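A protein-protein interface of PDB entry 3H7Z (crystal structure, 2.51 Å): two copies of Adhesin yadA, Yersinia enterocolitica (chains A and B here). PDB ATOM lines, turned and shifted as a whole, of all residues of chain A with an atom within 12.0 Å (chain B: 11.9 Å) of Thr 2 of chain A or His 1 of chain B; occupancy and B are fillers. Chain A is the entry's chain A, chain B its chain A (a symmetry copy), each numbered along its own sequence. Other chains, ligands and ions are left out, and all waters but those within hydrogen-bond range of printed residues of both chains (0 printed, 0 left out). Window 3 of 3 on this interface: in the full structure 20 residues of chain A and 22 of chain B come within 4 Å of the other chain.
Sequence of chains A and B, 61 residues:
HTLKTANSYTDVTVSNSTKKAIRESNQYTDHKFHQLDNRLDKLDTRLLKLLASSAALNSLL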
ATOM      1  N   HIS A   1       5.649  25.370 -13.149  1.00  0.00           N
ATOM      2  CA  HIS A   1       5.164  25.181 -14.526  1.00  0.00           C
ATOM      3  C   HIS A   1       6.373  25.443 -15.421  1.00  0.00           C
ATOM      4  O   HIS A   1       7.453  25.778 -14.939  1.00  0.00           O
ATOM      5  CB  HIS A   1       3.973  26.112 -14.780  1.00  0.00           C
ATOM      6  CG  HIS A   1       3.414  26.015 -16.160  1.00  0.00           C
ATOM      7  ND1 HIS A   1       2.430  26.859 -16.623  1.00  0.00           N
ATOM      8  CD2 HIS A   1       3.733  25.209 -17.203  1.00  0.00           C
ATOM      9  CE1 HIS A   1       2.165  26.574 -17.888  1.00  0.00           C
ATOM     10  NE2 HIS A   1       2.949  25.580 -18.265  1.00  0.00           N
ATOM     11  N   THR A   2       6.204  25.211 -16.712  1.00  0.00           N
ATOM     12  CA  THR A   2       7.173  25.529 -17.720  1.00  0.00           C
ATOM     13  C   THR A   2       7.224  27.038 -17.922  1.00  0.00           C
ATOM     14  O   THR A   2       8.241  27.547 -18.345  1.00  0.00           O
ATOM     15  CB  THR A   2       6.717  24.885 -19.031  1.00  0.00           C
ATOM     16  OG1 THR A   2       6.178  23.588 -18.742  1.00  0.00           O
ATOM     17  CG2 THR A   2       7.837  24.767 -20.035  1.00  0.00           C
ATOM     18  N   LEU A   3       6.107  27.727 -17.677  1.00  0.00           N
ATOM     19  CA  LEU A   3       6.063  29.175 -17.685  1.00  0.00           C
ATOM     20  C   LEU A   3       6.933  29.677 -16.576  1.00  0.00           C
ATOM     21  O   LEU A   3       7.962  30.235 -16.851  1.00  0.00           O
ATOM     22  CB  LEU A   3       4.670  29.717 -17.449  1.00  0.00           C
ATOM     23  CG  LEU A   3       3.846  30.336 -18.569  1.00  0.00           C
ATOM     24  CD1 LEU A   3       2.719  30.992 -17.860  1.00  0.00           C
ATOM     25  CD2 LEU A   3       4.575  31.346 -19.420  1.00  0.00           C
ATOM     26  N   LYS A   4       6.518  29.449 -15.333  1.00  0.00           N
ATOM     27  CA  LYS A   4       7.256  29.839 -14.135  1.00  0.00           C
ATOM     28  C   LYS A   4       8.754  29.731 -14.330  1.00  0.00           C
ATOM     29  O   LYS A   4       9.482  30.611 -13.937  1.00  0.00           O
ATOM     30  CB  LYS A   4       6.914  28.929 -12.951  1.00  0.00           C
ATOM     31  CG  LYS A   4       5.831  29.382 -11.995  1.00  0.00           C
ATOM     32  CD  LYS A   4       6.010  28.632 -10.665  1.00  0.00           C
ATOM     33  CE  LYS A   4       4.981  29.034  -9.623  1.00  0.00           C
ATOM     34  NZ  LYS A   4       5.386  28.512  -8.279  1.00  0.00           N
ATOM     35  N   THR A   5       9.209  28.629 -14.905  1.00  0.00           N
ATOM     36  CA  THR A   5      10.624  28.355 -15.053  1.00  0.00           C
ATOM     37  C   THR A   5      11.207  29.208 -16.174  1.00  0.00           C
ATOM     38  O   THR A   5      12.283  29.760 -16.041  1.00  0.00           O
ATOM     39  CB  THR A   5      10.836  26.868 -15.396  1.00  0.00           C
ATOM     40  OG1 THR A   5      10.357  26.064 -14.322  1.00  0.00           O
ATOM     41  CG2 THR A   5      12.270  26.568 -15.593  1.00  0.00           C
ATOM     42  N   ALA A   6      10.511  29.273 -17.299  1.00  0.00           N
ATOM     43  CA  ALA A   6      10.982  30.083 -18.374  1.00  0.00           C
ATOM     44  C   ALA A   6      11.003  31.498 -17.818  1.00  0.00           C
ATOM     45  O   ALA A   6      12.028  32.175 -17.853  1.00  0.00           O
ATOM     46  CB  ALA A   6      10.064  30.000 -19.540  1.00  0.00           C
ATOM     47  N   ASN A   7       9.863  31.915 -17.280  1.00  0.00           N
ATOM     48  CA  ASN A   7       9.684  33.243 -16.760  1.00  0.00           C
ATOM     49  C   ASN A   7      10.770  33.642 -15.784  1.00  0.00           C
ATOM     50  O   ASN A   7      11.216  34.773 -15.771  1.00  0.00           O
ATOM     51  CB  ASN A   7       8.297  33.405 -16.177  1.00  0.00           C
ATOM     52  CG  ASN A   7       7.285  33.851 -17.218  1.00  0.00           C
ATOM     53  OD1 ASN A   7       7.477  33.660 -18.398  1.00  0.00           O
ATOM     54  ND2 ASN A   7       6.209  34.469 -16.771  1.00  0.00           N
ATOM     55  N   SER A   8      11.258  32.707 -15.006  1.00  0.00           N
ATOM     56  CA  SER A   8      12.220  33.078 -14.024  1.00  0.00           C
ATOM     57  C   SER A   8      13.689  32.834 -14.472  1.00  0.00           C
ATOM     58  O   SER A   8      14.666  33.209 -13.799  1.00  0.00           O
ATOM     59  CB  SER A   8      11.821  32.471 -12.680  1.00  0.00           C
ATOM     60  OG  SER A   8      12.339  31.203 -12.558  1.00  0.00           O
ATOM     61  N   TYR A   9      13.833  32.228 -15.636  1.00  0.00           N
ATOM     62  CA  TYR A   9      15.065  32.235 -16.358  1.00  0.00           C
ATOM     63  C   TYR A   9      15.256  33.617 -16.967  1.00  0.00           C
ATOM     64  O   TYR A   9      16.361  34.071 -17.049  1.00  0.00           O
ATOM     65  CB  TYR A   9      14.973  31.236 -17.479  1.00  0.00           C
ATOM     66  CG  TYR A   9      16.165  31.161 -18.374  1.00  0.00           C
ATOM     67  CD1 TYR A   9      17.324  30.589 -17.951  1.00  0.00           C
ATOM     68  CD2 TYR A   9      16.107  31.587 -19.655  1.00  0.00           C
ATOM     69  CE1 TYR A   9      18.434  30.489 -18.775  1.00  0.00           C
ATOM     70  CE2 TYR A   9      17.207  31.482 -20.486  1.00  0.00           C
ATOM     71  CZ  TYR A   9      18.372  30.950 -20.022  1.00  0.00           C
ATOM     72  OH  TYR A   9      19.482  30.811 -20.846  1.00  0.00           O
ATOM     73  N   THR A  10      14.182  34.252 -17.430  1.00  0.00           N
ATOM     74  CA  THR A  10      14.221  35.595 -17.984  1.00  0.00           C
ATOM     75  C   THR A  10      14.538  36.562 -16.865  1.00  0.00           C
ATOM     76  O   THR A  10      15.488  37.312 -16.959  1.00  0.00           O
ATOM     77  CB  THR A  10      12.896  35.983 -18.641  1.00  0.00           C
ATOM     78  OG1 THR A  10      12.701  35.180 -19.812  1.00  0.00           O
ATOM     79  CG2 THR A  10      12.884  37.456 -19.040  1.00  0.00           C
ATOM     80  N   ASP A  11      13.748  36.534 -15.803  1.00  0.00           N
ATOM     81  CA  ASP A  11      14.106  37.230 -14.598  1.00  0.00           C
ATOM     82  C   ASP A  11      15.618  37.186 -14.301  1.00  0.00           C
ATOM     83  O   ASP A  11      16.287  38.181 -14.464  1.00  0.00           O
ATOM     84  CB  ASP A  11      13.273  36.688 -13.461  1.00  0.00           C
ATOM     85  CG  ASP A  11      11.821  37.102 -13.580  1.00  0.00           C
ATOM     86  OD1 ASP A  11      11.428  37.538 -14.671  1.00  0.00           O
ATOM     87  OD2 ASP A  11      11.071  36.996 -12.591  1.00  0.00           O
ATOM     88  N   HIS B   1      12.424  21.368 -26.284  1.00  0.00           N
ATOM     89  CA  HIS B   1      11.272  21.517 -25.380  1.00  0.00           C
ATOM     90  C   HIS B   1      10.765  22.942 -25.599  1.00  0.00           C
ATOM     91  O   HIS B   1      11.340  23.702 -26.376  1.00  0.00           O
ATOM     92  CB  HIS B   1      11.709  21.215 -23.941  1.00  0.00           C
ATOM     93  CG  HIS B   1      10.617  21.357 -22.936  1.00  0.00           C
ATOM     94  ND1 HIS B   1      10.838  21.256 -21.581  1.00  0.00           N
ATOM     95  CD2 HIS B   1       9.300  21.645 -23.076  1.00  0.00           C
ATOM     96  CE1 HIS B   1       9.705  21.471 -20.932  1.00  0.00           C
ATOM     97  NE2 HIS B   1       8.757  21.717 -21.819  1.00  0.00           N
ATOM     98  N   THR B   2       9.647  23.266 -24.973  1.00  0.00           N
ATOM     99  CA  THR B   2       9.097  24.589 -24.945  1.00  0.00           C
ATOM    100  C   THR B   2       9.945  25.478 -24.045  1.00  0.00           C
ATOM    101  O   THR B   2       9.958  26.676 -24.234  1.00  0.00           O
ATOM    102  CB  THR B   2       7.692  24.501 -24.344  1.00  0.00           C
ATOM    103  OG1 THR B   2       7.052  23.319 -24.843  1.00  0.00           O
ATOM    104  CG2 THR B   2       6.854  25.715 -24.661  1.00  0.00           C
ATOM    105  N   LEU B   3      10.595  24.889 -23.039  1.00  0.00           N
ATOM    106  CA  LEU B   3      11.549  25.591 -22.205  1.00  0.00           C
ATOM    107  C   LEU B   3      12.705  26.003 -23.062  1.00  0.00           C
ATOM    108  O   LEU B   3      12.861  27.170 -23.305  1.00  0.00           O
ATOM    109  CB  LEU B   3      12.097  24.726 -21.090  1.00  0.00           C
ATOM    110  CG  LEU B   3      11.677  24.919 -19.642  1.00  0.00           C
ATOM    111  CD1 LEU B   3      12.652  24.101 -18.877  1.00  0.00           C
ATOM    112  CD2 LEU B   3      11.703  26.344 -19.148  1.00  0.00           C
ATOM    113  N   LYS B   4      13.488  25.034 -23.528  1.00  0.00           N
ATOM    114  CA  LYS B   4      14.637  25.252 -24.402  1.00  0.00           C
ATOM    115  C   LYS B   4      14.406  26.396 -25.367  1.00  0.00           C
ATOM    116  O   LYS B   4      15.280  27.209 -25.563  1.00  0.00           O
ATOM    117  CB  LYS B   4      14.922  24.019 -25.264  1.00  0.00           C
ATOM    118  CG  LYS B   4      15.948  23.023 -24.764  1.00  0.00           C
ATOM    119  CD  LYS B   4      16.443  22.192 -25.958  1.00  0.00           C
ATOM    120  CE  LYS B   4      17.498  21.173 -25.565  1.00  0.00           C
ATOM    121  NZ  LYS B   4      18.154  20.620 -26.792  1.00  0.00           N
ATOM    122  N   THR B   5      13.243  26.431 -25.994  1.00  0.00           N
ATOM    123  CA  THR B   5      12.938  27.409 -27.020  1.00  0.00           C
ATOM    124  C   THR B   5      12.660  28.764 -26.382  1.00  0.00           C
ATOM    125  O   THR B   5      13.117  29.784 -26.863  1.00  0.00           O
ATOM    126  CB  THR B   5      11.693  26.966 -27.812  1.00  0.00           C
ATOM    127  OG1 THR B   5      11.968  25.732 -28.470  1.00  0.00           O
ATOM    128  CG2 THR B   5      11.336  27.966 -28.840  1.00  0.00           C
ATOM    129  N   ALA B   6      11.867  28.775 -25.321  1.00  0.00           N
ATOM    130  CA  ALA B   6      11.596  30.006 -24.655  1.00  0.00           C
ATOM    131  C   ALA B   6      12.950  30.492 -24.163  1.00  0.00           C
ATOM    132  O   ALA B   6      13.365  31.611 -24.458  1.00  0.00           O
ATOM    133  CB  ALA B   6      10.675  29.795 -23.507  1.00  0.00           C
ATOM    134  N   ASN B   7      13.639  29.620 -23.438  1.00  0.00           N
ATOM    135  CA  ASN B   7      14.910  29.929 -22.842  1.00  0.00           C
ATOM    136  C   ASN B   7      15.896  30.508 -23.834  1.00  0.00           C
ATOM    137  O   ASN B   7      16.653  31.404 -23.514  1.00  0.00           O
ATOM    138  CB  ASN B   7      15.465  28.724 -22.115  1.00  0.00           C
ATOM    139  CG  ASN B   7      14.991  28.655 -20.674  1.00  0.00           C
ATOM    140  OD1 ASN B   7      13.979  29.219 -20.321  1.00  0.00           O
ATOM    141  ND2 ASN B   7      15.743  27.971 -19.834  1.00  0.00           N
ATOM    142  N   SER B   8      15.854  30.056 -25.064  1.00  0.00           N
ATOM    143  CA  SER B   8      16.828  30.527 -25.991  1.00  0.00           C
ATOM    144  C   SER B   8      16.319  31.692 -26.886  1.00  0.00           C
ATOM    145  O   SER B   8      17.063  32.311 -27.667  1.00  0.00           O
ATOM    146  CB  SER B   8      17.435  29.333 -26.727  1.00  0.00           C
ATOM    147  OG  SER B   8      16.680  29.024 -27.834  1.00  0.00           O
ATOM    148  N   TYR B   9      15.044  32.004 -26.739  1.00  0.00           N
ATOM    149  CA  TYR B   9      14.498  33.240 -27.201  1.00  0.00           C
ATOM    150  C   TYR B   9      14.958  34.348 -26.263  1.00  0.00           C
ATOM    151  O   TYR B   9      15.188  35.434 -26.712  1.00  0.00           O
ATOM    152  CB  TYR B   9      12.997  33.160 -27.134  1.00  0.00           C
ATOM    153  CG  TYR B   9      12.268  34.400 -27.529  1.00  0.00           C
ATOM    154  CD1 TYR B   9      12.197  34.786 -28.831  1.00  0.00           C
ATOM    155  CD2 TYR B   9      11.592  35.136 -26.619  1.00  0.00           C
ATOM    156  CE1 TYR B   9      11.504  35.923 -29.220  1.00  0.00           C
ATOM    157  CE2 TYR B   9      10.893  36.265 -26.999  1.00  0.00           C
ATOM    158  CZ  TYR B   9      10.877  36.658 -28.305  1.00  0.00           C
ATOM    159  OH  TYR B   9      10.159  37.775 -28.715  1.00  0.00           O
ATOM    160  N   THR B  10      15.041  34.073 -24.963  1.00  0.00           N
ATOM    161  CA  THR B  10      15.517  35.025 -23.973  1.00  0.00           C
ATOM    162  C   THR B  10      16.993  35.256 -24.207  1.00  0.00           C
ATOM    163  O   THR B  10      17.412  36.383 -24.381  1.00  0.00           O
ATOM    164  CB  THR B  10      15.294  34.524 -22.544  1.00  0.00           C
ATOM    165  OG1 THR B  10      13.886  34.489 -22.276  1.00  0.00           O
ATOM    166  CG2 THR B  10      15.972  35.435 -21.526  1.00  0.00           C
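OG1 of Thr 10 of chain B lies within hydrogen-bond range of OG1 of Thr 10 of chain A.
OG1 of Thr 5 of chain A sits at hydrogen-bond distance from O of His 1 of chain A. O of His 1 of chain B lies within hydrogen-bond range of OG1 of Thr 5 of chain B.
His 1 of chain B touches Thr 2 of chain A (NE2 to CG2, 3.7 Å). Thr 2 of chain A touches Leu 3 of chain B (O to CD2, 3.8 Å). CD2 of Leu 3 of chain B touches CG2 of Thr 5 of chain A, 3.6 Å away. Leu 3 of chain B touches Ala 6 of chain A (CD2 to N, 3.7 Å). Ala 6 of chain A touches Asn 7 of chain B (CA to OD1, 3.7 Å). O of Asn 7 of chain B touches CE2 of Tyr 9 of chain A, at 3.1 Å.
Thr 2 of chain A touches two residues of chain B. No residue of chain B comes within 4 Å of Leu 3 of chain A. No residue of chain A comes within 4 Å of Thr 2 of chain B. Leu 3 of chain B touches just these residues of chain A: Thr 2 (3.8 Å), Thr 5 (3.6 Å) and Ala 6 (3.7 Å). No residue of chain A comes within 4 Å of Lys 4 of chain B. No residue of chain A comes within 4 Å of Thr 5 of chain B. Printed residues of chain B within 4 Å of Tyr 9 of chain A: Asn 7 (3.1 Å). Printed residues of chain A within 4 Å of Asn 7 of chain B: Ala 6 and Tyr 9. Ser 8 of chain B touches none of the printed residues of chain A. The nearest residue of chain B that does not touch Thr 2 of chain A is Thr 2 of chain B (4.3 Å). The nearest residue of chain A that does not touch His 1 of chain B is His 1 of chain A (7.6 Å).
Hydrophobic or aromatic side chains of chain B that line the printed part of chain A: His 1 and Leu 3. Printed residues of chain A that touch a printed residue of chain B: Thr 2, Thr 5, Ala 6, Tyr 9 and Thr 10. Hydrophobic or aromatic side chains of chain A that line the printed part of chain B: Tyr 9. Among the printed residues, 7 pairs touch across the chains. Among the printed residues, no Asp or Glu carboxylate lies within 4 Å of a Lys or Arg side-chain nitrogen of the other chain.
Thr 2 of chain A touches His 1 of chain B, but with the chains exchanged His 1 of chain A does not touch Thr 2 of chain B (7.5 Å). Thr 5 of chain A touches Leu 3 of chain B, but with the chains exchanged Leu 3 of chain A does not touch Thr 5 of chain B (10.7 Å). Ala 6 of chain A touches Asn 7 of chain B, but with the chains exchanged Asn 7 of chain A does not touch Ala 6 of chain B (6.6 Å). Tyr 9 of chain A touches Asn 7 of chain B, but with the chains exchanged Asn 7 of chain A does not touch Tyr 9 of chain B (9.3 Å). Positions printed for both chains: 1, 2, 3, 4, 5, 6, 7, 8, 9 and 10. Of the 7 pairs that touch across the chains among the printed residues, 1 has its exchanged pair printed and touching as well.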
